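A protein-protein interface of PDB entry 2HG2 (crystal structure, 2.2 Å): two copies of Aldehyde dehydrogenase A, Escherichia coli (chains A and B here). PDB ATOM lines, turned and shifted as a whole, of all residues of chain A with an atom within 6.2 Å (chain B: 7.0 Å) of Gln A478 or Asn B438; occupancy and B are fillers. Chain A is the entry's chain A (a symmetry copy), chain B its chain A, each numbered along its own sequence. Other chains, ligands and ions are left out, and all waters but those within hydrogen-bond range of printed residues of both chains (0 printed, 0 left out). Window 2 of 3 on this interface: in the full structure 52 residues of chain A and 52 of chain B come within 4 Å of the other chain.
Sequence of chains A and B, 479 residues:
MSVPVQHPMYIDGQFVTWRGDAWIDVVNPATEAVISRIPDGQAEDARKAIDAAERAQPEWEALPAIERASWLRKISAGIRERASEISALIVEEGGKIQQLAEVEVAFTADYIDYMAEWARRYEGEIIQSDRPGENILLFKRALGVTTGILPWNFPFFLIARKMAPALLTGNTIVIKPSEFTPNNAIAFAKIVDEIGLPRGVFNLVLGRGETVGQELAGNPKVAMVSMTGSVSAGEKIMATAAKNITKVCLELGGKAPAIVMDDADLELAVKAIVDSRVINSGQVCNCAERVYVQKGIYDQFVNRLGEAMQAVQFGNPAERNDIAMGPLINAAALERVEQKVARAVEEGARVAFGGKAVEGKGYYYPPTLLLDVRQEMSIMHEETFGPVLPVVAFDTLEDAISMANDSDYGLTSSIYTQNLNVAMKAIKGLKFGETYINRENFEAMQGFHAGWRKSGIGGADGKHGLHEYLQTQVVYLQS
The backbone carbonyl oxygen (O) of Tyr A476 is in hydrogen-bond range of the backbone NH (N) of Ile B437 (3.0 Å).
The backbone NH (N) of Gln A478 sits at hydrogen-bond distance from the backbone carbonyl oxygen (O) of Ile B437.
The side-chain carboxylate (OE2) of Glu A134 lies within salt-bridge range of the guanidinium group (NH1) of Arg B439, at 2.6 Å.
The side-chain carboxylate (OE2) of Glu B440 lies within salt-bridge range of the guanidinium group (NH1) of Arg A131 (2.7 Å).
NH2 of Arg A131 lies close to NH2 of Arg B439 (2.9 Å).
The backbone NH (N) of Ile B415 lies within hydrogen-bond range of the backbone carbonyl oxygen (O) of Tyr B436, at 2.9 Å.
O of Ile B415 lies within hydrogen-bond range of N of Asn B438, at 3.0 Å.
The backbone carbonyl oxygen (O) of Arg B439 sits at hydrogen-bond distance from the side-chain hydroxyl (OH) of Tyr B416, 3.1 Å away.
O of Thr B417 sits at hydrogen-bond distance from ND2 of Asn B438 (2.8 Å).
NH2 of Arg B439 lies within salt-bridge range of OE2 of Glu B440, 3.6 Å away.
The backbone carbonyl oxygen (O) of Pro A132 sits at hydrogen-bond distance from the side-chain amide nitrogen (NE2) of Gln A478, 3.3 Å away.
Tyr B436 touches Tyr A476.
NH1 of Arg B439 touches CD2 of Tyr A476, 3.6 Å away.
Ile B437 touches Leu A477 (CG2 to CD1, 3.7 Å).
Gln A478 touches Asn B438 (CB to O, 3.6 Å).
Gln A478 touches Arg B439.
Of the printed residues of chain B, Arg A131 touches Arg B439 and Glu B440.
Of the printed residues of chain A, Tyr B436 touches Tyr A476.
Asn B438 touches one residue of chain A.
The nearest residue of chain A that does not touch Asn B438 is Ser A479 (5.0 Å).
Hydrophobic or aromatic side chains of chain A within 4 Å of the printed part of chain B: Tyr A476 and Leu A477.
Printed residues of chain B that touch a printed residue of chain A: Tyr B436, Ile B437, Asn B438, Arg B439 and Glu B440.
Among the printed residues, 10 pairs touch across the chains.
No position is printed for both chains.
Of the 10 pairs that touch across the chains among the printed residues, none has its exchanged pair printed and touching as well.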
ATOM      1  N   ARG A 131       5.552   1.004  -3.689  1.00  0.00           N
ATOM      2  CA  ARG A 131       5.392  -0.431  -3.881  1.00  0.00           C
ATOM      3  C   ARG A 131       4.561  -1.054  -2.783  1.00  0.00           C
ATOM      4  O   ARG A 131       4.821  -0.838  -1.603  1.00  0.00           O
ATOM      5  CB  ARG A 131       6.747  -1.138  -3.902  1.00  0.00           C
ATOM      6  CG  ARG A 131       7.719  -0.594  -4.926  1.00  0.00           C
ATOM      7  CD  ARG A 131       8.894  -1.536  -5.086  1.00  0.00           C
ATOM      8  NE  ARG A 131       9.823  -1.052  -6.100  1.00  0.00           N
ATOM      9  CZ  ARG A 131      10.757  -1.802  -6.675  1.00  0.00           C
ATOM     10  NH1 ARG A 131      10.884  -3.078  -6.335  1.00  0.00           N
ATOM     11  NH2 ARG A 131      11.561  -1.275  -7.588  1.00  0.00           N
ATOM     12  N   PRO A 132       3.549  -1.850  -3.160  1.00  0.00           N
ATOM     13  CA  PRO A 132       2.658  -2.535  -2.219  1.00  0.00           C
ATOM     14  C   PRO A 132       3.455  -3.439  -1.275  1.00  0.00           C
ATOM     15  O   PRO A 132       4.307  -4.211  -1.720  1.00  0.00           O
ATOM     16  CB  PRO A 132       1.753  -3.357  -3.137  1.00  0.00           C
ATOM     17  CG  PRO A 132       1.720  -2.561  -4.393  1.00  0.00           C
ATOM     18  CD  PRO A 132       3.153  -2.127  -4.552  1.00  0.00           C
ATOM     19  N   GLY A 133       3.183  -3.328   0.022  1.00  0.00           N
ATOM     20  CA  GLY A 133       3.857  -4.172   0.998  1.00  0.00           C
ATOM     21  C   GLY A 133       5.301  -3.845   1.346  1.00  0.00           C
ATOM     22  O   GLY A 133       5.938  -4.582   2.105  1.00  0.00           O
ATOM     23  N   GLU A 134       5.831  -2.755   0.805  1.00  0.00           N
ATOM     24  CA  GLU A 134       7.206  -2.381   1.100  1.00  0.00           C
ATOM     25  C   GLU A 134       7.298  -1.296   2.171  1.00  0.00           C
ATOM     26  O   GLU A 134       6.479  -0.381   2.218  1.00  0.00           O
ATOM     27  CB  GLU A 134       7.913  -1.894  -0.171  1.00  0.00           C
ATOM     28  CG  GLU A 134       9.328  -1.365   0.072  1.00  0.00           C
ATOM     29  CD  GLU A 134      10.024  -0.877  -1.192  1.00  0.00           C
ATOM     30  OE1 GLU A 134       9.610   0.160  -1.751  1.00  0.00           O
ATOM     31  OE2 GLU A 134      10.993  -1.531  -1.629  1.00  0.00           O
ATOM     32  N   ASN A 135       8.293  -1.421   3.042  1.00  0.00           N
ATOM     33  CA  ASN A 135       8.544  -0.421   4.076  1.00  0.00           C
ATOM     34  C   ASN A 135       9.897   0.218   3.767  1.00  0.00           C
ATOM     35  O   ASN A 135      10.889  -0.488   3.539  1.00  0.00           O
ATOM     36  CB  ASN A 135       8.649  -1.054   5.467  1.00  0.00           C
ATOM     37  CG  ASN A 135       7.312  -1.501   6.021  1.00  0.00           C
ATOM     38  OD1 ASN A 135       6.385  -0.704   6.159  1.00  0.00           O
ATOM     39  ND2 ASN A 135       7.216  -2.784   6.357  1.00  0.00           N
ATOM     40  N   TYR A 476      15.162  -0.676   2.187  1.00  0.00           N
ATOM     41  CA  TYR A 476      13.954  -0.956   1.417  1.00  0.00           C
ATOM     42  C   TYR A 476      13.587  -2.407   1.718  1.00  0.00           C
ATOM     43  O   TYR A 476      14.119  -3.344   1.115  1.00  0.00           O
ATOM     44  CB  TYR A 476      14.205  -0.771  -0.086  1.00  0.00           C
ATOM     45  CG  TYR A 476      14.469   0.667  -0.514  1.00  0.00           C
ATOM     46  CD1 TYR A 476      15.734   1.244  -0.366  1.00  0.00           C
ATOM     47  CD2 TYR A 476      13.452   1.445  -1.077  1.00  0.00           C
ATOM     48  CE1 TYR A 476      15.980   2.554  -0.772  1.00  0.00           C
ATOM     49  CE2 TYR A 476      13.690   2.763  -1.483  1.00  0.00           C
ATOM     50  CZ  TYR A 476      14.958   3.308  -1.328  1.00  0.00           C
ATOM     51  OH  TYR A 476      15.207   4.597  -1.744  1.00  0.00           O
ATOM     52  N   LEU A 477      12.678  -2.590   2.668  1.00  0.00           N
ATOM     53  CA  LEU A 477      12.267  -3.923   3.082  1.00  0.00           C
ATOM     54  C   LEU A 477      11.011  -4.390   2.360  1.00  0.00           C
ATOM     55  O   LEU A 477       9.903  -3.944   2.663  1.00  0.00           O
ATOM     56  CB  LEU A 477      12.062  -3.933   4.601  1.00  0.00           C
ATOM     57  CG  LEU A 477      11.647  -5.227   5.299  1.00  0.00           C
ATOM     58  CD1 LEU A 477      12.437  -6.405   4.762  1.00  0.00           C
ATOM     59  CD2 LEU A 477      11.876  -5.065   6.789  1.00  0.00           C
ATOM     60  N   GLN A 478      11.197  -5.296   1.405  1.00  0.00           N
ATOM     61  CA  GLN A 478      10.091  -5.812   0.608  1.00  0.00           C
ATOM     62  C   GLN A 478       9.417  -7.034   1.225  1.00  0.00           C
ATOM     63  O   GLN A 478      10.049  -8.078   1.419  1.00  0.00           O
ATOM     64  CB  GLN A 478      10.576  -6.159  -0.799  1.00  0.00           C
ATOM     65  CG  GLN A 478       9.456  -6.552  -1.751  1.00  0.00           C
ATOM     66  CD  GLN A 478       8.540  -5.388  -2.076  1.00  0.00           C
ATOM     67  OE1 GLN A 478       8.932  -4.454  -2.784  1.00  0.00           O
ATOM     68  NE2 GLN A 478       7.317  -5.429  -1.553  1.00  0.00           N
ATOM     69  N   SER A 479       8.126  -6.890   1.515  1.00  0.00           N
ATOM     70  CA  SER A 479       7.323  -7.955   2.105  1.00  0.00           C
ATOM     71  C   SER A 479       7.945  -8.477   3.401  1.00  0.00           C
ATOM     72  O   SER A 479       7.496  -8.019   4.474  1.00  0.00           O
ATOM     73  CB  SER A 479       7.160  -9.102   1.099  1.00  0.00           C
ATOM     74  OG  SER A 479       6.404 -10.173   1.639  1.00  0.00           O
ATOM     75  OXT SER A 479       8.878  -9.318   3.333  1.00  0.00           O
ATOM     76  N   ASP B 263      18.488 -19.692   2.947  1.00  0.00           N
ATOM     77  CA  ASP B 263      17.038 -19.631   3.069  1.00  0.00           C
ATOM     78  C   ASP B 263      16.449 -18.532   2.197  1.00  0.00           C
ATOM     79  O   ASP B 263      15.391 -17.987   2.501  1.00  0.00           O
ATOM     80  CB  ASP B 263      16.651 -19.393   4.530  1.00  0.00           C
ATOM     81  CG  ASP B 263      16.965 -17.980   4.996  1.00  0.00           C
ATOM     82  OD1 ASP B 263      18.047 -17.463   4.640  1.00  0.00           O
ATOM     83  OD2 ASP B 263      16.136 -17.390   5.727  1.00  0.00           O
ATOM     84  N   ALA B 264      17.130 -18.214   1.106  1.00  0.00           N
ATOM     85  CA  ALA B 264      16.661 -17.169   0.207  1.00  0.00           C
ATOM     86  C   ALA B 264      15.747 -17.721  -0.871  1.00  0.00           C
ATOM     87  O   ALA B 264      15.813 -18.902  -1.212  1.00  0.00           O
ATOM     88  CB  ALA B 264      17.846 -16.469  -0.445  1.00  0.00           C
ATOM     89  N   ASP B 265      14.883 -16.861  -1.395  1.00  0.00           N
ATOM     90  CA  ASP B 265      13.988 -17.249  -2.471  1.00  0.00           C
ATOM     91  C   ASP B 265      14.894 -17.228  -3.692  1.00  0.00           C
ATOM     92  O   ASP B 265      15.093 -16.183  -4.315  1.00  0.00           O
ATOM     93  CB  ASP B 265      12.863 -16.227  -2.639  1.00  0.00           C
ATOM     94  CG  ASP B 265      11.855 -16.634  -3.704  1.00  0.00           C
ATOM     95  OD1 ASP B 265      12.273 -16.946  -4.844  1.00  0.00           O
ATOM     96  OD2 ASP B 265      10.642 -16.633  -3.400  1.00  0.00           O
ATOM     97  N   LEU B 268      13.668 -15.459  -6.925  1.00  0.00           N
ATOM     98  CA  LEU B 268      13.617 -14.008  -6.763  1.00  0.00           C
ATOM     99  C   LEU B 268      15.008 -13.377  -6.769  1.00  0.00           C
ATOM    100  O   LEU B 268      15.256 -12.393  -7.467  1.00  0.00           O
ATOM    101  CB  LEU B 268      12.897 -13.664  -5.457  1.00  0.00           C
ATOM    102  CG  LEU B 268      13.016 -12.238  -4.912  1.00  0.00           C
ATOM    103  CD1 LEU B 268      12.594 -11.214  -5.967  1.00  0.00           C
ATOM    104  CD2 LEU B 268      12.156 -12.124  -3.661  1.00  0.00           C
ATOM    105  N   ALA B 269      15.915 -13.954  -5.989  1.00  0.00           N
ATOM    106  CA  ALA B 269      17.279 -13.450  -5.896  1.00  0.00           C
ATOM    107  C   ALA B 269      17.994 -13.405  -7.243  1.00  0.00           C
ATOM    108  O   ALA B 269      18.602 -12.394  -7.590  1.00  0.00           O
ATOM    109  CB  ALA B 269      18.081 -14.297  -4.912  1.00  0.00           C
ATOM    110  N   ALA B 272      16.582 -10.582  -9.371  1.00  0.00           N
ATOM    111  CA  ALA B 272      16.963  -9.276  -8.853  1.00  0.00           C
ATOM    112  C   ALA B 272      18.414  -8.939  -9.194  1.00  0.00           C
ATOM    113  O   ALA B 272      18.702  -7.856  -9.702  1.00  0.00           O
ATOM    114  CB  ALA B 272      16.747  -9.231  -7.340  1.00  0.00           C
ATOM    115  N   SER B 414      22.573  -5.213  -0.654  1.00  0.00           N
ATOM    116  CA  SER B 414      21.342  -5.996  -0.720  1.00  0.00           C
ATOM    117  C   SER B 414      21.503  -7.367  -0.076  1.00  0.00           C
ATOM    118  O   SER B 414      22.609  -7.903   0.000  1.00  0.00           O
ATOM    119  CB  SER B 414      20.900  -6.167  -2.175  1.00  0.00           C
ATOM    120  OG  SER B 414      21.829  -6.942  -2.911  1.00  0.00           O
ATOM    121  N   ILE B 415      20.397  -7.931   0.394  1.00  0.00           N
ATOM    122  CA  ILE B 415      20.429  -9.249   1.008  1.00  0.00           C
ATOM    123  C   ILE B 415      19.104  -9.977   0.803  1.00  0.00           C
ATOM    124  O   ILE B 415      18.036  -9.356   0.781  1.00  0.00           O
ATOM    125  CB  ILE B 415      20.748  -9.165   2.516  1.00  0.00           C
ATOM    126  CG1 ILE B 415      20.941 -10.577   3.079  1.00  0.00           C
ATOM    127  CG2 ILE B 415      19.643  -8.422   3.253  1.00  0.00           C
ATOM    128  CD1 ILE B 415      21.437 -10.621   4.517  1.00  0.00           C
ATOM    129  N   TYR B 416      19.182 -11.294   0.635  1.00  0.00           N
ATOM    130  CA  TYR B 416      17.994 -12.115   0.423  1.00  0.00           C
ATOM    131  C   TYR B 416      17.937 -13.209   1.472  1.00  0.00           C
ATOM    132  O   TYR B 416      18.836 -14.043   1.562  1.00  0.00           O
ATOM    133  CB  TYR B 416      18.017 -12.719  -0.981  1.00  0.00           C
ATOM    134  CG  TYR B 416      18.215 -11.671  -2.047  1.00  0.00           C
ATOM    135  CD1 TYR B 416      19.477 -11.125  -2.286  1.00  0.00           C
ATOM    136  CD2 TYR B 416      17.129 -11.158  -2.757  1.00  0.00           C
ATOM    137  CE1 TYR B 416      19.654 -10.088  -3.201  1.00  0.00           C
ATOM    138  CE2 TYR B 416      17.294 -10.118  -3.674  1.00  0.00           C
ATOM    139  CZ  TYR B 416      18.559  -9.587  -3.887  1.00  0.00           C
ATOM    140  OH  TYR B 416      18.727  -8.537  -4.759  1.00  0.00           O
ATOM    141  N   THR B 417      16.875 -13.192   2.270  1.00  0.00           N
ATOM    142  CA  THR B 417      16.689 -14.167   3.336  1.00  0.00           C
ATOM    143  C   THR B 417      15.232 -14.123   3.783  1.00  0.00           C
ATOM    144  O   THR B 417      14.480 -13.233   3.377  1.00  0.00           O
ATOM    145  CB  THR B 417      17.587 -13.833   4.553  1.00  0.00           C
ATOM    146  OG1 THR B 417      17.483 -14.874   5.531  1.00  0.00           O
ATOM    147  CG2 THR B 417      17.152 -12.513   5.196  1.00  0.00           C
ATOM    148  N   GLN B 418      14.834 -15.080   4.618  1.00  0.00           N
ATOM    149  CA  GLN B 418      13.467 -15.115   5.116  1.00  0.00           C
ATOM    150  C   GLN B 418      13.437 -15.173   6.644  1.00  0.00           C
ATOM    151  O   GLN B 418      12.365 -15.252   7.251  1.00  0.00           O
ATOM    152  CB  GLN B 418      12.726 -16.310   4.518  1.00  0.00           C
ATOM    153  CG  GLN B 418      12.902 -16.415   3.009  1.00  0.00           C
ATOM    154  CD  GLN B 418      12.080 -17.532   2.390  1.00  0.00           C
ATOM    155  OE1 GLN B 418      12.076 -18.666   2.878  1.00  0.00           O
ATOM    156  NE2 GLN B 418      11.388 -17.217   1.297  1.00  0.00           N
ATOM    157  N   ASN B 419      14.617 -15.122   7.261  1.00  0.00           N
ATOM    158  CA  ASN B 419      14.725 -15.164   8.719  1.00  0.00           C
ATOM    159  C   ASN B 419      14.692 -13.747   9.315  1.00  0.00           C
ATOM    160  O   ASN B 419      15.380 -12.844   8.834  1.00  0.00           O
ATOM    161  CB  ASN B 419      16.012 -15.889   9.118  1.00  0.00           C
ATOM    162  CG  ASN B 419      16.163 -16.032  10.628  1.00  0.00           C
ATOM    163  OD1 ASN B 419      16.613 -15.110  11.315  1.00  0.00           O
ATOM    164  ND2 ASN B 419      15.772 -17.190  11.151  1.00  0.00           N
ATOM    165  N   ALA B 423      17.763 -10.740   8.867  1.00  0.00           N
ATOM    166  CA  ALA B 423      17.396  -9.459   8.283  1.00  0.00           C
ATOM    167  C   ALA B 423      17.818  -8.299   9.179  1.00  0.00           C
ATOM    168  O   ALA B 423      18.534  -7.405   8.738  1.00  0.00           O
ATOM    169  CB  ALA B 423      15.889  -9.412   8.036  1.00  0.00           C
ATOM    170  N   TYR B 436      18.903  -3.061   0.282  1.00  0.00           N
ATOM    171  CA  TYR B 436      17.688  -3.608  -0.292  1.00  0.00           C
ATOM    172  C   TYR B 436      17.515  -5.022   0.218  1.00  0.00           C
ATOM    173  O   TYR B 436      18.469  -5.805   0.242  1.00  0.00           O
ATOM    174  CB  TYR B 436      17.767  -3.608  -1.815  1.00  0.00           C
ATOM    175  CG  TYR B 436      17.763  -2.223  -2.396  1.00  0.00           C
ATOM    176  CD1 TYR B 436      18.948  -1.500  -2.530  1.00  0.00           C
ATOM    177  CD2 TYR B 436      16.567  -1.611  -2.771  1.00  0.00           C
ATOM    178  CE1 TYR B 436      18.941  -0.204  -3.019  1.00  0.00           C
ATOM    179  CE2 TYR B 436      16.548  -0.311  -3.258  1.00  0.00           C
ATOM    180  CZ  TYR B 436      17.738   0.387  -3.378  1.00  0.00           C
ATOM    181  OH  TYR B 436      17.728   1.683  -3.838  1.00  0.00           O
ATOM    182  N   ILE B 437      16.302  -5.349   0.639  1.00  0.00           N
ATOM    183  CA  ILE B 437      16.035  -6.680   1.155  1.00  0.00           C
ATOM    184  C   ILE B 437      14.958  -7.383   0.341  1.00  0.00           C
ATOM    185  O   ILE B 437      13.828  -6.900   0.241  1.00  0.00           O
ATOM    186  CB  ILE B 437      15.615  -6.615   2.636  1.00  0.00           C
ATOM    187  CG1 ILE B 437      16.726  -5.944   3.450  1.00  0.00           C
ATOM    188  CG2 ILE B 437      15.338  -8.013   3.165  1.00  0.00           C
ATOM    189  CD1 ILE B 437      16.402  -5.769   4.917  1.00  0.00           C
ATOM    190  N   ASN B 438      15.332  -8.519  -0.245  1.00  0.00           N
ATOM    191  CA  ASN B 438      14.446  -9.336  -1.068  1.00  0.00           C
ATOM    192  C   ASN B 438      13.780  -8.594  -2.216  1.00  0.00           C
ATOM    193  O   ASN B 438      12.576  -8.732  -2.438  1.00  0.00           O
ATOM    194  CB  ASN B 438      13.382 -10.005  -0.195  1.00  0.00           C
ATOM    195  CG  ASN B 438      13.982 -10.970   0.811  1.00  0.00           C
ATOM    196  OD1 ASN B 438      14.903 -11.721   0.488  1.00  0.00           O
ATOM    197  ND2 ASN B 438      13.455 -10.963   2.033  1.00  0.00           N
ATOM    198  N   ARG B 439      14.574  -7.814  -2.942  1.00  0.00           N
ATOM    199  CA  ARG B 439      14.113  -7.049  -4.102  1.00  0.00           C
ATOM    200  C   ARG B 439      15.332  -6.474  -4.828  1.00  0.00           C
ATOM    201  O   ARG B 439      16.438  -6.509  -4.297  1.00  0.00           O
ATOM    202  CB  ARG B 439      13.167  -5.914  -3.685  1.00  0.00           C
ATOM    203  CG  ARG B 439      13.771  -4.891  -2.730  1.00  0.00           C
ATOM    204  CD  ARG B 439      13.105  -3.511  -2.885  1.00  0.00           C
ATOM    205  NE  ARG B 439      13.525  -2.850  -4.118  1.00  0.00           N
ATOM    206  CZ  ARG B 439      13.236  -1.593  -4.452  1.00  0.00           C
ATOM    207  NH1 ARG B 439      12.510  -0.823  -3.649  1.00  0.00           N
ATOM    208  NH2 ARG B 439      13.694  -1.097  -5.599  1.00  0.00           N
ATOM    209  N   GLU B 440      15.135  -5.942  -6.032  1.00  0.00           N
ATOM    210  CA  GLU B 440      16.252  -5.385  -6.798  1.00  0.00           C
ATOM    211  C   GLU B 440      16.584  -3.941  -6.420  1.00  0.00           C
ATOM    212  O   GLU B 440      15.736  -3.213  -5.906  1.00  0.00           O
ATOM    213  CB  GLU B 440      15.970  -5.477  -8.301  1.00  0.00           C
ATOM    214  CG  GLU B 440      14.955  -4.489  -8.840  1.00  0.00           C
ATOM    215  CD  GLU B 440      13.574  -4.690  -8.263  1.00  0.00           C
ATOM    216  OE1 GLU B 440      13.162  -5.858  -8.098  1.00  0.00           O
ATOM    217  OE2 GLU B 440      12.895  -3.680  -7.988  1.00  0.00           O
